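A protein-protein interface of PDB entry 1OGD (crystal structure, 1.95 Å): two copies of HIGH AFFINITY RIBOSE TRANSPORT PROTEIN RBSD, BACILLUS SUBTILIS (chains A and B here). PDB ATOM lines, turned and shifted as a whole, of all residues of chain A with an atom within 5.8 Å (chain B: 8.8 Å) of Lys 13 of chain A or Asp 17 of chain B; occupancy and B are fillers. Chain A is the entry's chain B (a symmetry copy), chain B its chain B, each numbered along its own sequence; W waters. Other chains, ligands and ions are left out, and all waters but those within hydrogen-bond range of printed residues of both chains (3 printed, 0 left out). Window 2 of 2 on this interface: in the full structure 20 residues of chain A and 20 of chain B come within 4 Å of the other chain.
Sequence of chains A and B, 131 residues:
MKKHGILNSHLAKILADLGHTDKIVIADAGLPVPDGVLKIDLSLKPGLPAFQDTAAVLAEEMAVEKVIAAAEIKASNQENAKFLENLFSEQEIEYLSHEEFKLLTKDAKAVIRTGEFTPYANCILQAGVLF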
ATOM      1  N   ASN A   8      -1.832 -17.352   4.173  1.00  0.00           N
ATOM      2  CA  ASN A   8      -2.365 -16.177   4.849  1.00  0.00           C
ATOM      3  C   ASN A   8      -1.411 -14.987   4.748  1.00  0.00           C
ATOM      4  O   ASN A   8      -0.260 -15.066   5.175  1.00  0.00           O
ATOM      5  CB  ASN A   8      -2.650 -16.502   6.312  1.00  0.00           C
ATOM      6  CG  ASN A   8      -3.389 -15.388   7.012  1.00  0.00           C
ATOM      7  OD1 ASN A   8      -2.790 -14.392   7.424  1.00  0.00           O
ATOM      8  ND2 ASN A   8      -4.708 -15.537   7.133  1.00  0.00           N
ATOM      9  N   SER A   9      -1.904 -13.891   4.180  1.00  0.00           N
ATOM     10  CA  SER A   9      -1.097 -12.687   4.006  1.00  0.00           C
ATOM     11  C   SER A   9      -0.617 -12.089   5.332  1.00  0.00           C
ATOM     12  O   SER A   9       0.535 -11.659   5.429  1.00  0.00           O
ATOM     13  CB  SER A   9      -1.872 -11.638   3.200  1.00  0.00           C
ATOM     14  OG  SER A   9      -3.096 -11.303   3.829  1.00  0.00           O
ATOM     15  N   HIS A  10      -1.483 -12.062   6.348  1.00  0.00           N
ATOM     16  CA  HIS A  10      -1.097 -11.514   7.658  1.00  0.00           C
ATOM     17  C   HIS A  10       0.038 -12.332   8.281  1.00  0.00           C
ATOM     18  O   HIS A  10       1.010 -11.777   8.801  1.00  0.00           O
ATOM     19  CB  HIS A  10      -2.280 -11.512   8.643  1.00  0.00           C
ATOM     20  CG  HIS A  10      -3.507 -10.826   8.127  1.00  0.00           C
ATOM     21  ND1 HIS A  10      -3.486  -9.548   7.611  1.00  0.00           N
ATOM     22  CD2 HIS A  10      -4.797 -11.239   8.060  1.00  0.00           C
ATOM     23  CE1 HIS A  10      -4.708  -9.203   7.245  1.00  0.00           C
ATOM     24  NE2 HIS A  10      -5.523 -10.211   7.507  1.00  0.00           N
ATOM     25  N   LEU A  11      -0.088 -13.656   8.226  1.00  0.00           N
ATOM     26  CA  LEU A  11       0.925 -14.530   8.806  1.00  0.00           C
ATOM     27  C   LEU A  11       2.241 -14.519   8.027  1.00  0.00           C
ATOM     28  O   LEU A  11       3.320 -14.600   8.624  1.00  0.00           O
ATOM     29  CB  LEU A  11       0.393 -15.959   8.915  1.00  0.00           C
ATOM     30  CG  LEU A  11      -0.749 -16.161   9.918  1.00  0.00           C
ATOM     31  CD1 LEU A  11      -1.184 -17.618   9.917  1.00  0.00           C
ATOM     32  CD2 LEU A  11      -0.288 -15.752  11.305  1.00  0.00           C
ATOM     33  N   ALA A  12       2.145 -14.422   6.702  1.00  0.00           N
ATOM     34  CA  ALA A  12       3.338 -14.397   5.855  1.00  0.00           C
ATOM     35  C   ALA A  12       4.214 -13.215   6.261  1.00  0.00           C
ATOM     36  O   ALA A  12       5.439 -13.314   6.267  1.00  0.00           O
ATOM     37  CB  ALA A  12       2.945 -14.274   4.382  1.00  0.00           C
ATOM     38  N   LYS A  13       3.578 -12.099   6.608  1.00  0.00           N
ATOM     39  CA  LYS A  13       4.315 -10.900   7.015  1.00  0.00           C
ATOM     40  C   LYS A  13       5.046 -11.092   8.339  1.00  0.00           C
ATOM     41  O   LYS A  13       6.156 -10.601   8.512  1.00  0.00           O
ATOM     42  CB  LYS A  13       3.366  -9.708   7.107  1.00  0.00           C
ATOM     43  CG  LYS A  13       2.713  -9.368   5.780  1.00  0.00           C
ATOM     44  CD  LYS A  13       1.730  -8.223   5.914  1.00  0.00           C
ATOM     45  CE  LYS A  13       1.148  -7.865   4.563  1.00  0.00           C
ATOM     46  NZ  LYS A  13       0.043  -6.893   4.689  1.00  0.00           N
ATOM     47  N   ILE A  14       4.421 -11.801   9.273  1.00  0.00           N
ATOM     48  CA  ILE A  14       5.031 -12.061  10.574  1.00  0.00           C
ATOM     49  C   ILE A  14       6.186 -13.049  10.447  1.00  0.00           C
ATOM     50  O   ILE A  14       7.225 -12.884  11.078  1.00  0.00           O
ATOM     51  CB  ILE A  14       4.007 -12.645  11.552  1.00  0.00           C
ATOM     52  CG1 ILE A  14       2.907 -11.623  11.802  1.00  0.00           C
ATOM     53  CG2 ILE A  14       4.691 -13.043  12.857  1.00  0.00           C
ATOM     54  CD1 ILE A  14       1.864 -12.120  12.733  1.00  0.00           C
ATOM     55  N   LEU A  15       6.001 -14.085   9.638  1.00  0.00           N
ATOM     56  CA  LEU A  15       7.064 -15.069   9.457  1.00  0.00           C
ATOM     57  C   LEU A  15       8.273 -14.433   8.774  1.00  0.00           C
ATOM     58  O   LEU A  15       9.416 -14.773   9.081  1.00  0.00           O
ATOM     59  CB  LEU A  15       6.570 -16.260   8.623  1.00  0.00           C
ATOM     60  CG  LEU A  15       5.481 -17.122   9.269  1.00  0.00           C
ATOM     61  CD1 LEU A  15       5.192 -18.344   8.393  1.00  0.00           C
ATOM     62  CD2 LEU A  15       5.937 -17.551  10.651  1.00  0.00           C
ATOM     63  N   ALA A  16       8.013 -13.504   7.858  1.00  0.00           N
ATOM     64  CA  ALA A  16       9.077 -12.830   7.120  1.00  0.00           C
ATOM     65  C   ALA A  16      10.051 -12.093   8.031  1.00  0.00           C
ATOM     66  O   ALA A  16      11.235 -11.988   7.717  1.00  0.00           O
ATOM     67  CB  ALA A  16       8.480 -11.865   6.121  1.00  0.00           C
ATOM     68  N   ASP A  17       9.557 -11.589   9.159  1.00  0.00           N
ATOM     69  CA  ASP A  17      10.403 -10.854  10.091  1.00  0.00           C
ATOM     70  C   ASP A  17      11.010 -11.671  11.227  1.00  0.00           C
ATOM     71  O   ASP A  17      11.748 -11.125  12.045  1.00  0.00           O
ATOM     72  CB  ASP A  17       9.629  -9.676  10.695  1.00  0.00           C
ATOM     73  CG  ASP A  17       9.513  -8.505   9.742  1.00  0.00           C
ATOM     74  OD1 ASP A  17      10.465  -8.283   8.958  1.00  0.00           O
ATOM     75  OD2 ASP A  17       8.481  -7.800   9.787  1.00  0.00           O
ATOM     76  N   LYS B   2      11.374 -18.264   8.572  1.00  0.00           N
ATOM     77  CA  LYS B   2      10.433 -18.681   7.544  1.00  0.00           C
ATOM     78  C   LYS B   2      11.154 -19.688   6.649  1.00  0.00           C
ATOM     79  O   LYS B   2      12.223 -19.397   6.115  1.00  0.00           O
ATOM     80  CB  LYS B   2       9.992 -17.449   6.740  1.00  0.00           C
ATOM     81  CG  LYS B   2       8.961 -17.699   5.658  1.00  0.00           C
ATOM     82  CD  LYS B   2       8.354 -16.380   5.164  1.00  0.00           C
ATOM     83  CE  LYS B   2       9.356 -15.520   4.410  1.00  0.00           C
ATOM     84  NZ  LYS B   2       9.582 -16.009   3.027  1.00  0.00           N
ATOM     85  N   ASN B   8      13.843 -11.885   1.287  1.00  0.00           N
ATOM     86  CA  ASN B   8      13.690 -10.504   1.727  1.00  0.00           C
ATOM     87  C   ASN B   8      12.358 -10.284   2.443  1.00  0.00           C
ATOM     88  O   ASN B   8      11.293 -10.525   1.876  1.00  0.00           O
ATOM     89  CB  ASN B   8      13.809  -9.561   0.533  1.00  0.00           C
ATOM     90  CG  ASN B   8      13.860  -8.112   0.951  1.00  0.00           C
ATOM     91  OD1 ASN B   8      12.829  -7.501   1.241  1.00  0.00           O
ATOM     92  ND2 ASN B   8      15.070  -7.555   1.009  1.00  0.00           N
ATOM     93  N   SER B   9      12.434  -9.828   3.689  1.00  0.00           N
ATOM     94  CA  SER B   9      11.239  -9.588   4.492  1.00  0.00           C
ATOM     95  C   SER B   9      10.314  -8.525   3.891  1.00  0.00           C
ATOM     96  O   SER B   9       9.092  -8.698   3.907  1.00  0.00           O
ATOM     97  CB  SER B   9      11.630  -9.203   5.925  1.00  0.00           C
ATOM     98  OG  SER B   9      12.454  -8.051   5.944  1.00  0.00           O
ATOM     99  N   HIS B  10      10.881  -7.440   3.360  1.00  0.00           N
ATOM    100  CA  HIS B  10      10.062  -6.378   2.754  1.00  0.00           C
ATOM    101  C   HIS B  10       9.289  -6.907   1.542  1.00  0.00           C
ATOM    102  O   HIS B  10       8.096  -6.637   1.382  1.00  0.00           O
ATOM    103  CB  HIS B  10      10.927  -5.192   2.287  1.00  0.00           C
ATOM    104  CG  HIS B  10      11.818  -4.626   3.348  1.00  0.00           C
ATOM    105  ND1 HIS B  10      11.352  -4.246   4.589  1.00  0.00           N
ATOM    106  CD2 HIS B  10      13.149  -4.366   3.349  1.00  0.00           C
ATOM    107  CE1 HIS B  10      12.356  -3.777   5.310  1.00  0.00           C
ATOM    108  NE2 HIS B  10      13.457  -3.839   4.581  1.00  0.00           N
ATOM    109  N   LEU B  11       9.974  -7.665   0.688  1.00  0.00           N
ATOM    110  CA  LEU B  11       9.341  -8.206  -0.509  1.00  0.00           C
ATOM    111  C   LEU B  11       8.316  -9.297  -0.201  1.00  0.00           C
ATOM    112  O   LEU B  11       7.283  -9.391  -0.874  1.00  0.00           O
ATOM    113  CB  LEU B  11      10.400  -8.738  -1.474  1.00  0.00           C
ATOM    114  CG  LEU B  11      11.311  -7.677  -2.102  1.00  0.00           C
ATOM    115  CD1 LEU B  11      12.316  -8.344  -3.028  1.00  0.00           C
ATOM    116  CD2 LEU B  11      10.472  -6.676  -2.873  1.00  0.00           C
ATOM    117  N   ALA B  12       8.605 -10.116   0.809  1.00  0.00           N
ATOM    118  CA  ALA B  12       7.695 -11.194   1.196  1.00  0.00           C
ATOM    119  C   ALA B  12       6.341 -10.596   1.567  1.00  0.00           C
ATOM    120  O   ALA B  12       5.296 -11.170   1.267  1.00  0.00           O
ATOM    121  CB  ALA B  12       8.264 -11.974   2.383  1.00  0.00           C
ATOM    122  N   LYS B  13       6.365  -9.433   2.214  1.00  0.00           N
ATOM    123  CA  LYS B  13       5.127  -8.766   2.622  1.00  0.00           C
ATOM    124  C   LYS B  13       4.315  -8.273   1.430  1.00  0.00           C
ATOM    125  O   LYS B  13       3.091  -8.338   1.442  1.00  0.00           O
ATOM    126  CB  LYS B  13       5.443  -7.601   3.558  1.00  0.00           C
ATOM    127  CG  LYS B  13       6.123  -8.043   4.841  1.00  0.00           C
ATOM    128  CD  LYS B  13       6.483  -6.863   5.722  1.00  0.00           C
ATOM    129  CE  LYS B  13       7.096  -7.341   7.021  1.00  0.00           C
ATOM    130  NZ  LYS B  13       7.638  -6.216   7.809  1.00  0.00           N
ATOM    131  N   ILE B  14       4.998  -7.775   0.403  1.00  0.00           N
ATOM    132  CA  ILE B  14       4.326  -7.287  -0.799  1.00  0.00           C
ATOM    133  C   ILE B  14       3.746  -8.443  -1.607  1.00  0.00           C
ATOM    134  O   ILE B  14       2.639  -8.352  -2.126  1.00  0.00           O
ATOM    135  CB  ILE B  14       5.299  -6.517  -1.696  1.00  0.00           C
ATOM    136  CG1 ILE B  14       5.793  -5.280  -0.959  1.00  0.00           C
ATOM    137  CG2 ILE B  14       4.621  -6.138  -3.008  1.00  0.00           C
ATOM    138  CD1 ILE B  14       6.756  -4.482  -1.759  1.00  0.00           C
ATOM    139  N   LEU B  15       4.501  -9.529  -1.724  1.00  0.00           N
ATOM    140  CA  LEU B  15       4.012 -10.681  -2.475  1.00  0.00           C
ATOM    141  C   LEU B  15       2.796 -11.296  -1.783  1.00  0.00           C
ATOM    142  O   LEU B  15       1.872 -11.768  -2.444  1.00  0.00           O
ATOM    143  CB  LEU B  15       5.110 -11.743  -2.625  1.00  0.00           C
ATOM    144  CG  LEU B  15       6.321 -11.337  -3.470  1.00  0.00           C
ATOM    145  CD1 LEU B  15       7.259 -12.534  -3.649  1.00  0.00           C
ATOM    146  CD2 LEU B  15       5.843 -10.826  -4.815  1.00  0.00           C
ATOM    147  N   ALA B  16       2.802 -11.276  -0.453  1.00  0.00           N
ATOM    148  CA  ALA B  16       1.710 -11.845   0.331  1.00  0.00           C
ATOM    149  C   ALA B  16       0.364 -11.199   0.024  1.00  0.00           C
ATOM    150  O   ALA B  16      -0.671 -11.857   0.096  1.00  0.00           O
ATOM    151  CB  ALA B  16       2.013 -11.718   1.806  1.00  0.00           C
ATOM    152  N   ASP B  17       0.378  -9.915  -0.324  1.00  0.00           N
ATOM    153  CA  ASP B  17      -0.857  -9.200  -0.624  1.00  0.00           C
ATOM    154  C   ASP B  17      -1.258  -9.150  -2.094  1.00  0.00           C
ATOM    155  O   ASP B  17      -2.295  -8.580  -2.425  1.00  0.00           O
ATOM    156  CB  ASP B  17      -0.785  -7.765  -0.087  1.00  0.00           C
ATOM    157  CG  ASP B  17      -1.002  -7.692   1.409  1.00  0.00           C
ATOM    158  OD1 ASP B  17      -1.794  -8.508   1.933  1.00  0.00           O
ATOM    159  OD2 ASP B  17      -0.397  -6.809   2.057  1.00  0.00           O
ATOM    160  N   LEU B  18      -0.452  -9.737  -2.976  1.00  0.00           N
ATOM    161  CA  LEU B  18      -0.763  -9.717  -4.406  1.00  0.00           C
ATOM    162  C   LEU B  18      -2.003 -10.511  -4.784  1.00  0.00           C
ATOM    163  O   LEU B  18      -2.185 -11.648  -4.356  1.00  0.00           O
ATOM    164  CB  LEU B  18       0.410 -10.253  -5.244  1.00  0.00           C
ATOM    165  CG  LEU B  18       1.715  -9.453  -5.336  1.00  0.00           C
ATOM    166  CD1 LEU B  18       2.677 -10.207  -6.230  1.00  0.00           C
ATOM    167  CD2 LEU B  18       1.458  -8.052  -5.898  1.00  0.00           C
ATOM    168  N   GLY B  19      -2.848  -9.886  -5.595  1.00  0.00           N
ATOM    169  CA  GLY B  19      -4.043 -10.535  -6.094  1.00  0.00           C
ATOM    170  C   GLY B  19      -3.897 -10.520  -7.606  1.00  0.00           C
ATOM    171  O   GLY B  19      -2.989  -9.871  -8.123  1.00  0.00           O
ATOM    172  N   HIS B  20      -4.770 -11.221  -8.319  1.00  0.00           N
ATOM    173  CA  HIS B  20      -4.702 -11.262  -9.778  1.00  0.00           C
ATOM    174  C   HIS B  20      -4.674  -9.856 -10.393  1.00  0.00           C
ATOM    175  O   HIS B  20      -5.522  -9.020 -10.089  1.00  0.00           O
ATOM    176  CB  HIS B  20      -5.903 -12.036 -10.334  1.00  0.00           C
ATOM    177  CG  HIS B  20      -5.786 -12.372 -11.790  1.00  0.00           C
ATOM    178  ND1 HIS B  20      -6.863 -12.774 -12.549  1.00  0.00           N
ATOM    179  CD2 HIS B  20      -4.716 -12.382 -12.621  1.00  0.00           C
ATOM    180  CE1 HIS B  20      -6.464 -13.013 -13.786  1.00  0.00           C
ATOM    181  NE2 HIS B  20      -5.165 -12.783 -13.856  1.00  0.00           N
ATOM    182  N   ASP B  22      -2.396  -7.486  -9.949  1.00  0.00           N
ATOM    183  CA  ASP B  22      -1.654  -6.463  -9.211  1.00  0.00           C
ATOM    184  C   ASP B  22      -0.267  -6.362  -9.848  1.00  0.00           C
ATOM    185  O   ASP B  22       0.247  -7.346 -10.384  1.00  0.00           O
ATOM    186  CB  ASP B  22      -1.500  -6.828  -7.735  1.00  0.00           C
ATOM    187  CG  ASP B  22      -2.784  -6.642  -6.946  1.00  0.00           C
ATOM    188  OD1 ASP B  22      -3.680  -5.902  -7.407  1.00  0.00           O
ATOM    189  OD2 ASP B  22      -2.882  -7.230  -5.853  1.00  0.00           O
ATOM    190  N   LYS B  23       0.344  -5.185  -9.779  1.00  0.00           N
ATOM    191  CA  LYS B  23       1.650  -4.979 -10.393  1.00  0.00           C
ATOM    192  C   LYS B  23       2.740  -4.488  -9.445  1.00  0.00           C
ATOM    193  O   LYS B  23       2.475  -3.727  -8.507  1.00  0.00           O
ATOM    194  CB  LYS B  23       1.512  -3.975 -11.538  1.00  0.00           C
ATOM    195  CG  LYS B  23       0.433  -4.342 -12.545  1.00  0.00           C
ATOM    196  CD  LYS B  23       0.097  -3.175 -13.452  1.00  0.00           C
ATOM    197  CE  LYS B  23      -1.113  -3.494 -14.315  1.00  0.00           C
ATOM    198  NZ  LYS B  23      -2.285  -3.903 -13.480  1.00  0.00           N
ATOM    199  N   ILE B  24       3.966  -4.946  -9.694  1.00  0.00           N
ATOM    200  CA  ILE B  24       5.127  -4.516  -8.925  1.00  0.00           C
ATOM    201  C   ILE B  24       6.156  -4.117  -9.979  1.00  0.00           C
ATOM    202  O   ILE B  24       6.135  -4.639 -11.098  1.00  0.00           O
ATOM    203  CB  ILE B  24       5.723  -5.631  -8.040  1.00  0.00           C
ATOM    204  CG1 ILE B  24       6.216  -6.786  -8.908  1.00  0.00           C
ATOM    205  CG2 ILE B  24       4.685  -6.109  -7.031  1.00  0.00           C
ATOM    206  CD1 ILE B  24       6.975  -7.842  -8.127  1.00  0.00           C
ATOM    207  N   LYS B 109       2.094  -1.606  -6.738  1.00  0.00           N
ATOM    208  CA  LYS B 109       2.018  -1.796  -5.299  1.00  0.00           C
ATOM    209  C   LYS B 109       3.380  -1.468  -4.695  1.00  0.00           C
ATOM    210  O   LYS B 109       3.494  -1.188  -3.511  1.00  0.00           O
ATOM    211  CB  LYS B 109       1.649  -3.250  -4.972  1.00  0.00           C
ATOM    212  CG  LYS B 109       0.340  -3.714  -5.578  1.00  0.00           C
ATOM    213  CD  LYS B 109      -0.847  -2.943  -5.020  1.00  0.00           C
ATOM    214  CE  LYS B 109      -2.126  -3.292  -5.773  1.00  0.00           C
ATOM    215  NZ  LYS B 109      -3.287  -2.464  -5.343  1.00  0.00           N
ATOM    216  N   ALA B 127       0.838  -9.684 -11.731  1.00  0.00           N
ATOM    217  CA  ALA B 127       0.473 -10.923 -11.057  1.00  0.00           C
ATOM    218  C   ALA B 127      -0.579 -11.767 -11.759  1.00  0.00           C
ATOM    219  O   ALA B 127      -1.574 -11.254 -12.278  1.00  0.00           O
ATOM    220  CB  ALA B 127       0.015 -10.612  -9.630  1.00  0.00           C
HETATM  221  O   HOH W   1      12.159 -15.307   8.694  1.00  0.00           O
HETATM  222  O   HOH W   2      10.777  -6.240   7.314  1.00  0.00           O
HETATM  223  O   HOH W   3      -2.635  -8.584   4.436  1.00  0.00           O
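Of the 10 printed residues of chain A, 6 touch a printed residue of chain B. Printed residues of chain A that touch a printed residue of chain B: Ser 9, Ala 12, Lys 13, Leu 15, Ala 16 and Asp 17. Hydrophobic or aromatic side chains of chain A that line the printed part of chain B: Ala 12, Leu 15 and Ala 16. Printed residues of chain B that touch a printed residue of chain A: Lys 2, Ser 9, Ala 12, Lys 13, Ala 16 and Asp 17. Hydrophobic or aromatic side chains of chain B that line the printed part of chain A: Ala 12 and Ala 16. Along chain B the printed residues that touch a printed residue of chain A span positions 2 to 17. Among the printed residues, 11 pairs touch across the chains. Among the printed residues, Asp or Glu carboxylates within 4 Å of a Lys or Arg side-chain nitrogen of the other chain: Lys 13 of chain A with Asp 17 of chain B and Asp 17 of chain A with Lys 13 of chain B.
Ser 9 of chain A touches Asp 17 of chain B, and with the chains exchanged Asp 17 of chain A touches Ser 9 of chain B. Ala 12 of chain A touches Ala 16 of chain B, and with the chains exchanged Ala 16 of chain A touches Ala 12 of chain B. Lys 13 of chain B touches its own counterpart, Lys 13 of chain A. Lys 13 of chain A touches Asp 17 of chain B, and with the chains exchanged Asp 17 of chain A touches Lys 13 of chain B.
Ala 16 of chain B touches Ser 9 of chain A. Asp 17 of chain B touches Ser 9 of chain A. Ala 12 of chain A touches Ala 16 of chain B. Lys 13 of chain B touches Lys 13 of chain A (CE to O, 3.7 Å). Leu 15 of chain A touches Lys 2 of chain B (O to CB, 3.6 Å). CA of Ala 16 of chain A touches CE of Lys 2 of chain B (3.8 Å). O of Ala 16 of chain A touches CB of Ser 9 of chain B, 3.3 Å away. CB of Ala 12 of chain B touches CB of Ala 16 of chain A (3.7 Å). CB of Ser 9 of chain B touches OD1 of Asp 17 of chain A, 3.4 Å away.
Water W3 lies within hydrogen-bond range of OD1 of Asp 17 of chain B (2.6 Å), OG of Ser 9 of chain A (2.8 Å), NZ of Lys 13 of chain A (3.2 Å) and ND1 of His 10 of chain A (3.4 Å). Water W2 lies within hydrogen-bond range of OD1 of Asp 17 of chain A, OG of Ser 9 of chain B, NZ of Lys 13 of chain B and ND1 of His 10 of chain B. Water W1 bridges the backbone carbonyl oxygen (O) of Leu 15 of chain A and the backbone NH (N) of Lys 2 of chain B.
Of chain B, only Lys 13 (3.7 Å) and Asp 17 (2.7 Å) come within 4 Å of Lys 13 of chain A. Asp 17 of chain B touches just these residues of chain A: Ser 9 (3.4 Å) and Lys 13 (2.7 Å). Of the printed residues of chain B, Ala 12 of chain A touches Ala 16 (3.7 Å). Printed residues of chain A within 4 Å of Ala 12 of chain B: Ala 16 (3.7 Å). Printed residues of chain B within 4 Å of Leu 15 of chain A: Lys 2. Of the printed residues of chain B, Ser 9 of chain A touches Ala 16 and Asp 17. Of the printed residues of chain A, Lys 13 of chain B touches Lys 13 (3.7 Å) and Asp 17 (2.7 Å). Printed residues of chain A within 4 Å of Ser 9 of chain B: Ala 16 (3.3 Å) and Asp 17 (3.4 Å). Ile 14 of chain A touches none of the printed residues of chain B. Gly 19 of chain B touches none of the printed residues of chain A.
OD2 of Asp 17 of chain A is in salt-bridge range of NZ of Lys 13 of chain B (2.7 Å). OD2 of Asp 17 of chain B is in salt-bridge range of NZ of Lys 13 of chain A (2.7 Å).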
